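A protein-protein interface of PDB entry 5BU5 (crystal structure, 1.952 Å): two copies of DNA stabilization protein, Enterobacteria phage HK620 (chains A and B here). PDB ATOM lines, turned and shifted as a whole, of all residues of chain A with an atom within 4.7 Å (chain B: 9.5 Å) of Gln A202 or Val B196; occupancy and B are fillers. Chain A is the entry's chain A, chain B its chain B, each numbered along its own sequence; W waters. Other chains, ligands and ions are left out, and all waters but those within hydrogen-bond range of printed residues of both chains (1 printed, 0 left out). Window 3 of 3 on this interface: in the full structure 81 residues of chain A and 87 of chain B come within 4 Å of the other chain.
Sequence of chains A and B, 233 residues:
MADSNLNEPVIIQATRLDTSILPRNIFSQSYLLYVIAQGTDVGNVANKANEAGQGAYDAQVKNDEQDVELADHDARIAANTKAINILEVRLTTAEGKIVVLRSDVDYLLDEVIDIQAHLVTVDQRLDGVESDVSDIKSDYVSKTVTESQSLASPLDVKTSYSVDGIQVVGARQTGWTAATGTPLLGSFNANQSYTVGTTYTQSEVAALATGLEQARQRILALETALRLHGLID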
ATOM      1  N   TYR A 200     -27.476 -10.476 -20.275  1.00  0.00           N
ATOM      2  CA  TYR A 200     -26.236 -10.781 -19.583  1.00  0.00           C
ATOM      3  C   TYR A 200     -26.088  -9.914 -18.342  1.00  0.00           C
ATOM      4  O   TYR A 200     -26.160  -8.687 -18.413  1.00  0.00           O
ATOM      5  CB  TYR A 200     -25.026 -10.594 -20.501  1.00  0.00           C
ATOM      6  CG  TYR A 200     -23.704 -10.855 -19.808  1.00  0.00           C
ATOM      7  CD1 TYR A 200     -23.187 -12.142 -19.710  1.00  0.00           C
ATOM      8  CD2 TYR A 200     -22.974  -9.813 -19.252  1.00  0.00           C
ATOM      9  CE1 TYR A 200     -21.979 -12.380 -19.073  1.00  0.00           C
ATOM     10  CE2 TYR A 200     -21.772 -10.044 -18.612  1.00  0.00           C
ATOM     11  CZ  TYR A 200     -21.278 -11.324 -18.528  1.00  0.00           C
ATOM     12  OH  TYR A 200     -20.079 -11.541 -17.895  1.00  0.00           O
ATOM     13  N   THR A 201     -25.880 -10.565 -17.207  1.00  0.00           N
ATOM     14  CA  THR A 201     -25.619  -9.876 -15.957  1.00  0.00           C
ATOM     15  C   THR A 201     -24.357 -10.483 -15.376  1.00  0.00           C
ATOM     16  O   THR A 201     -24.321 -11.681 -15.095  1.00  0.00           O
ATOM     17  CB  THR A 201     -26.785 -10.009 -14.960  1.00  0.00           C
ATOM     18  OG1 THR A 201     -28.007  -9.602 -15.587  1.00  0.00           O
ATOM     19  CG2 THR A 201     -26.535  -9.147 -13.727  1.00  0.00           C
ATOM     20  N   GLN A 202     -23.323  -9.661 -15.227  1.00  0.00           N
ATOM     21  CA  GLN A 202     -22.020 -10.126 -14.771  1.00  0.00           C
ATOM     22  C   GLN A 202     -22.142 -10.901 -13.461  1.00  0.00           C
ATOM     23  O   GLN A 202     -21.541 -11.961 -13.302  1.00  0.00           O
ATOM     24  CB  GLN A 202     -21.055  -8.948 -14.608  1.00  0.00           C
ATOM     25  CG  GLN A 202     -19.761  -9.295 -13.882  1.00  0.00           C
ATOM     26  CD  GLN A 202     -18.800  -8.120 -13.807  1.00  0.00           C
ATOM     27  OE1 GLN A 202     -19.214  -6.971 -13.651  1.00  0.00           O
ATOM     28  NE2 GLN A 202     -17.508  -8.405 -13.934  1.00  0.00           N
ATOM     29  N   SER A 203     -22.939 -10.373 -12.536  1.00  0.00           N
ATOM     30  CA  SER A 203     -23.102 -10.980 -11.218  1.00  0.00           C
ATOM     31  C   SER A 203     -23.754 -12.366 -11.270  1.00  0.00           C
ATOM     32  O   SER A 203     -23.445 -13.232 -10.449  1.00  0.00           O
ATOM     33  CB  SER A 203     -23.912 -10.052 -10.309  1.00  0.00           C
ATOM     34  OG  SER A 203     -25.212  -9.825 -10.829  1.00  0.00           O
ATOM     35  N   GLU A 204     -24.652 -12.575 -12.228  1.00  0.00           N
ATOM     36  CA  GLU A 204     -25.321 -13.867 -12.367  1.00  0.00           C
ATOM     37  C   GLU A 204     -24.362 -14.939 -12.884  1.00  0.00           C
ATOM     38  O   GLU A 204     -24.323 -16.060 -12.367  1.00  0.00           O
ATOM     39  CB  GLU A 204     -26.537 -13.746 -13.288  1.00  0.00           C
ATOM     40  CG  GLU A 204     -27.654 -12.891 -12.703  1.00  0.00           C
ATOM     41  CD  GLU A 204     -28.858 -12.775 -13.620  1.00  0.00           C
ATOM     42  OE1 GLU A 204     -28.735 -13.118 -14.814  1.00  0.00           O
ATOM     43  OE2 GLU A 204     -29.927 -12.341 -13.143  1.00  0.00           O
ATOM     44  N   VAL A 205     -23.587 -14.595 -13.906  1.00  0.00           N
ATOM     45  CA  VAL A 205     -22.610 -15.527 -14.448  1.00  0.00           C
ATOM     46  C   VAL A 205     -21.464 -15.700 -13.450  1.00  0.00           C
ATOM     47  O   VAL A 205     -20.869 -16.770 -13.352  1.00  0.00           O
ATOM     48  CB  VAL A 205     -22.073 -15.058 -15.807  1.00  0.00           C
ATOM     49  CG1 VAL A 205     -21.106 -16.082 -16.381  1.00  0.00           C
ATOM     50  CG2 VAL A 205     -23.228 -14.829 -16.769  1.00  0.00           C
ATOM     51  N   ALA A 206     -21.175 -14.645 -12.694  1.00  0.00           N
ATOM     52  CA  ALA A 206     -20.164 -14.715 -11.644  1.00  0.00           C
ATOM     53  C   ALA A 206     -20.617 -15.644 -10.522  1.00  0.00           C
ATOM     54  O   ALA A 206     -19.795 -16.287  -9.871  1.00  0.00           O
ATOM     55  CB  ALA A 206     -19.860 -13.332 -11.095  1.00  0.00           C
ATOM     56  N   ALA A 209     -19.782 -18.968 -11.719  1.00  0.00           N
ATOM     57  CA  ALA A 209     -18.351 -19.174 -11.553  1.00  0.00           C
ATOM     58  C   ALA A 209     -18.026 -19.520 -10.107  1.00  0.00           C
ATOM     59  O   ALA A 209     -17.293 -20.470  -9.840  1.00  0.00           O
ATOM     60  CB  ALA A 209     -17.579 -17.940 -11.996  1.00  0.00           C
ATOM     61  N   SER B 193      -9.524 -20.290 -11.213  1.00  0.00           N
ATOM     62  CA  SER B 193     -10.460 -19.191 -11.070  1.00  0.00           C
ATOM     63  C   SER B 193     -11.029 -18.856 -12.434  1.00  0.00           C
ATOM     64  O   SER B 193     -10.293 -18.787 -13.416  1.00  0.00           O
ATOM     65  CB  SER B 193      -9.776 -17.970 -10.454  1.00  0.00           C
ATOM     66  OG  SER B 193     -10.727 -16.996 -10.062  1.00  0.00           O
ATOM     67  N   TYR B 194     -12.339 -18.650 -12.502  1.00  0.00           N
ATOM     68  CA  TYR B 194     -12.974 -18.350 -13.777  1.00  0.00           C
ATOM     69  C   TYR B 194     -13.364 -16.884 -13.847  1.00  0.00           C
ATOM     70  O   TYR B 194     -14.249 -16.427 -13.126  1.00  0.00           O
ATOM     71  CB  TYR B 194     -14.195 -19.242 -13.985  1.00  0.00           C
ATOM     72  CG  TYR B 194     -13.853 -20.710 -13.940  1.00  0.00           C
ATOM     73  CD1 TYR B 194     -13.310 -21.347 -15.046  1.00  0.00           C
ATOM     74  CD2 TYR B 194     -14.053 -21.453 -12.787  1.00  0.00           C
ATOM     75  CE1 TYR B 194     -12.981 -22.686 -15.009  1.00  0.00           C
ATOM     76  CE2 TYR B 194     -13.727 -22.799 -12.741  1.00  0.00           C
ATOM     77  CZ  TYR B 194     -13.194 -23.407 -13.856  1.00  0.00           C
ATOM     78  OH  TYR B 194     -12.868 -24.742 -13.823  1.00  0.00           O
ATOM     79  N   THR B 195     -12.696 -16.156 -14.737  1.00  0.00           N
ATOM     80  CA  THR B 195     -12.942 -14.733 -14.910  1.00  0.00           C
ATOM     81  C   THR B 195     -14.288 -14.488 -15.571  1.00  0.00           C
ATOM     82  O   THR B 195     -14.605 -15.087 -16.597  1.00  0.00           O
ATOM     83  CB  THR B 195     -11.840 -14.067 -15.756  1.00  0.00           C
ATOM     84  OG1 THR B 195     -10.560 -14.321 -15.167  1.00  0.00           O
ATOM     85  CG2 THR B 195     -12.063 -12.565 -15.840  1.00  0.00           C
ATOM     86  N   VAL B 196     -15.079 -13.604 -14.973  1.00  0.00           N
ATOM     87  CA  VAL B 196     -16.348 -13.198 -15.553  1.00  0.00           C
ATOM     88  C   VAL B 196     -16.369 -11.677 -15.636  1.00  0.00           C
ATOM     89  O   VAL B 196     -16.394 -10.989 -14.618  1.00  0.00           O
ATOM     90  CB  VAL B 196     -17.548 -13.698 -14.729  1.00  0.00           C
ATOM     91  CG1 VAL B 196     -18.848 -13.170 -15.316  1.00  0.00           C
ATOM     92  CG2 VAL B 196     -17.560 -15.221 -14.677  1.00  0.00           C
ATOM     93  N   GLY B 197     -16.376 -11.156 -16.858  1.00  0.00           N
ATOM     94  CA  GLY B 197     -16.236  -9.729 -17.064  1.00  0.00           C
ATOM     95  C   GLY B 197     -17.561  -9.004 -17.012  1.00  0.00           C
ATOM     96  O   GLY B 197     -18.622  -9.629 -16.986  1.00  0.00           O
ATOM     97  N   THR B 198     -17.489  -7.677 -16.979  1.00  0.00           N
ATOM     98  CA  THR B 198     -18.672  -6.827 -17.036  1.00  0.00           C
ATOM     99  C   THR B 198     -19.575  -7.207 -18.203  1.00  0.00           C
ATOM    100  O   THR B 198     -20.799  -7.154 -18.099  1.00  0.00           O
ATOM    101  CB  THR B 198     -18.287  -5.344 -17.159  1.00  0.00           C
ATOM    102  OG1 THR B 198     -17.561  -5.139 -18.377  1.00  0.00           O
ATOM    103  CG2 THR B 198     -17.417  -4.922 -15.982  1.00  0.00           C
ATOM    104  N   THR B 199     -18.960  -7.550 -19.326  1.00  0.00           N
ATOM    105  CA  THR B 199     -19.701  -7.896 -20.529  1.00  0.00           C
ATOM    106  C   THR B 199     -19.442  -9.314 -21.031  1.00  0.00           C
ATOM    107  O   THR B 199     -18.419  -9.920 -20.708  1.00  0.00           O
ATOM    108  CB  THR B 199     -19.416  -6.886 -21.606  1.00  0.00           C
ATOM    109  OG1 THR B 199     -18.001  -6.809 -21.819  1.00  0.00           O
ATOM    110  CG2 THR B 199     -19.943  -5.546 -21.123  1.00  0.00           C
ATOM    111  N   TYR B 200     -20.383  -9.836 -21.815  1.00  0.00           N
ATOM    112  CA  TYR B 200     -20.320 -11.216 -22.290  1.00  0.00           C
ATOM    113  C   TYR B 200     -19.122 -11.488 -23.194  1.00  0.00           C
ATOM    114  O   TYR B 200     -18.912 -10.807 -24.198  1.00  0.00           O
ATOM    115  CB  TYR B 200     -21.610 -11.584 -23.033  1.00  0.00           C
ATOM    116  CG  TYR B 200     -21.633 -13.013 -23.540  1.00  0.00           C
ATOM    117  CD1 TYR B 200     -22.056 -14.050 -22.716  1.00  0.00           C
ATOM    118  CD2 TYR B 200     -21.235 -13.326 -24.834  1.00  0.00           C
ATOM    119  CE1 TYR B 200     -22.080 -15.356 -23.166  1.00  0.00           C
ATOM    120  CE2 TYR B 200     -21.256 -14.633 -25.291  1.00  0.00           C
ATOM    121  CZ  TYR B 200     -21.680 -15.643 -24.452  1.00  0.00           C
ATOM    122  OH  TYR B 200     -21.706 -16.945 -24.897  1.00  0.00           O
ATOM    123  N   THR B 201     -18.348 -12.501 -22.815  1.00  0.00           N
ATOM    124  CA  THR B 201     -17.208 -12.971 -23.592  1.00  0.00           C
ATOM    125  C   THR B 201     -17.300 -14.479 -23.774  1.00  0.00           C
ATOM    126  O   THR B 201     -17.285 -15.225 -22.791  1.00  0.00           O
ATOM    127  CB  THR B 201     -15.872 -12.627 -22.914  1.00  0.00           C
ATOM    128  OG1 THR B 201     -15.829 -11.225 -22.620  1.00  0.00           O
ATOM    129  CG2 THR B 201     -14.706 -12.997 -23.821  1.00  0.00           C
ATOM    130  N   SER B 203     -15.288 -16.819 -24.705  1.00  0.00           N
ATOM    131  CA  SER B 203     -14.190 -17.613 -24.166  1.00  0.00           C
ATOM    132  C   SER B 203     -14.289 -17.783 -22.654  1.00  0.00           C
ATOM    133  O   SER B 203     -13.893 -18.816 -22.115  1.00  0.00           O
ATOM    134  CB  SER B 203     -12.846 -16.978 -24.522  1.00  0.00           C
ATOM    135  OG  SER B 203     -12.730 -15.689 -23.945  1.00  0.00           O
ATOM    136  N   GLU B 204     -14.812 -16.767 -21.975  1.00  0.00           N
ATOM    137  CA  GLU B 204     -14.957 -16.815 -20.523  1.00  0.00           C
ATOM    138  C   GLU B 204     -16.047 -17.795 -20.106  1.00  0.00           C
ATOM    139  O   GLU B 204     -15.854 -18.595 -19.195  1.00  0.00           O
ATOM    140  CB  GLU B 204     -15.259 -15.421 -19.966  1.00  0.00           C
ATOM    141  CG  GLU B 204     -14.115 -14.433 -20.122  1.00  0.00           C
ATOM    142  CD  GLU B 204     -14.444 -13.064 -19.560  1.00  0.00           C
ATOM    143  OE1 GLU B 204     -15.637 -12.798 -19.298  1.00  0.00           O
ATOM    144  OE2 GLU B 204     -13.510 -12.252 -19.384  1.00  0.00           O
ATOM    145  N   VAL B 205     -17.192 -17.730 -20.779  1.00  0.00           N
ATOM    146  CA  VAL B 205     -18.298 -18.635 -20.492  1.00  0.00           C
ATOM    147  C   VAL B 205     -17.941 -20.039 -20.958  1.00  0.00           C
ATOM    148  O   VAL B 205     -18.361 -21.031 -20.357  1.00  0.00           O
ATOM    149  CB  VAL B 205     -19.603 -18.167 -21.162  1.00  0.00           C
ATOM    150  CG1 VAL B 205     -20.753 -19.099 -20.809  1.00  0.00           C
ATOM    151  CG2 VAL B 205     -19.926 -16.750 -20.734  1.00  0.00           C
ATOM    152  N   ALA B 206     -17.139 -20.117 -22.016  1.00  0.00           N
ATOM    153  CA  ALA B 206     -16.647 -21.397 -22.514  1.00  0.00           C
ATOM    154  C   ALA B 206     -15.713 -22.035 -21.493  1.00  0.00           C
ATOM    155  O   ALA B 206     -15.639 -23.262 -21.388  1.00  0.00           O
ATOM    156  CB  ALA B 206     -15.938 -21.223 -23.846  1.00  0.00           C
ATOM    157  N   ALA B 207     -14.997 -21.200 -20.747  1.00  0.00           N
ATOM    158  CA  ALA B 207     -14.122 -21.693 -19.692  1.00  0.00           C
ATOM    159  C   ALA B 207     -14.951 -22.319 -18.574  1.00  0.00           C
ATOM    160  O   ALA B 207     -14.543 -23.322 -17.981  1.00  0.00           O
ATOM    161  CB  ALA B 207     -13.247 -20.571 -19.151  1.00  0.00           C
ATOM    162  N   LEU B 208     -16.118 -21.733 -18.303  1.00  0.00           N
ATOM    163  CA  LEU B 208     -17.056 -22.295 -17.331  1.00  0.00           C
ATOM    164  C   LEU B 208     -17.582 -23.647 -17.779  1.00  0.00           C
ATOM    165  O   LEU B 208     -17.648 -24.585 -16.987  1.00  0.00           O
ATOM    166  CB  LEU B 208     -18.238 -21.353 -17.083  1.00  0.00           C
ATOM    167  CG  LEU B 208     -18.113 -20.230 -16.050  1.00  0.00           C
ATOM    168  CD1 LEU B 208     -17.859 -20.830 -14.685  1.00  0.00           C
ATOM    169  CD2 LEU B 208     -17.027 -19.231 -16.395  1.00  0.00           C
HETATM  170  O   HOH W   1     -18.207 -12.908 -19.499  1.00  0.00           O
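The backbone carbonyl oxygen (O) of Gly B197 sits at hydrogen-bond distance from the side-chain hydroxyl (OH) of Tyr A200.
O of Val B196 is in hydrogen-bond range of NE2 of Gln A202 (2.9 Å).
The backbone carbonyl oxygen (O) of Gly B197 sits close to the side-chain amide nitrogen (NE2) of Gln A202, at 3.5 Å.
NE2 of Gln A202 sits close to N of Thr B198.
N of Gly B197 is in hydrogen-bond range of OE1 of Glu B204 (3.0 Å).
O of Thr B199 sits at hydrogen-bond distance from OG1 of Thr B201, 3.5 Å away.
Among the printed residues, merely in contact across the chains: Tyr A200 with Val B196, Tyr A200 with Thr B198, Tyr A200 with Thr B199, Tyr A200 with Tyr B200, Val A205 with Val B196, Ala A206 with Val B196, Ala A209 with Tyr B194, Ala A209 with Val B196 and Ala A209 with Leu B208.
Gln A202 touches just these residues of chain B: Val B196 (2.9 Å), Gly B197 (3.1 Å) and Thr B198 (3.1 Å).
Val B196 touches just these residues of chain A: Tyr A200, Gln A202, Val A205, Ala A206 and Ala A209.
No residue of chain B comes within 4 Å of Thr A201.
No residue of chain B comes within 4 Å of Ser A203.
Of the printed residues of chain B, Val A205 touches Val B196 (3.8 Å).
Ala A206 touches just one residue of chain B: Val B196 (3.8 Å).
Of the printed residues of chain A, Tyr B200 touches Tyr A200 (3.5 Å).
Of the printed residues of chain B, Tyr A200 touches Val B196 (3.3 Å), Gly B197 (2.6 Å), Thr B198 (3.1 Å), Thr B199 (3.4 Å) and Tyr B200 (3.5 Å).
Of the printed residues of chain A, Thr B198 touches Tyr A200 (3.1 Å) and Gln A202 (3.1 Å).
The nearest residue of chain B that does not touch Gln A202 is Thr B199 (5.3 Å).
The nearest printed residue of chain A that does not touch Val B196 is Thr A201 (5.7 Å).
The nearest printed residue of chain A that does not touch Tyr B200 is Val A205 (6.1 Å).
Printed residues of chain A that touch a printed residue of chain B: Tyr A200, Gln A202, Val A205, Ala A206 and Ala A209.
Among the printed residues, 13 pairs touch across the chains.
Among the printed residues, no Asp or Glu carboxylate lies within 4 Å of a Lys or Arg side-chain nitrogen of the other chain.
Tyr A200 touches its own counterpart, Tyr B200.
Of the 13 pairs that touch across the chains among the printed residues, 1 has its exchanged pair printed and touching as well.
Water W1 lies within hydrogen-bond range of the side-chain carboxylate of Glu B204 (2.6 Å), the side-chain hydroxyl of Tyr A200 (2.8 Å), the backbone carbonyl oxygen of Thr B199 (3.2 Å) and the backbone NH of Thr B201 (3.3 Å).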
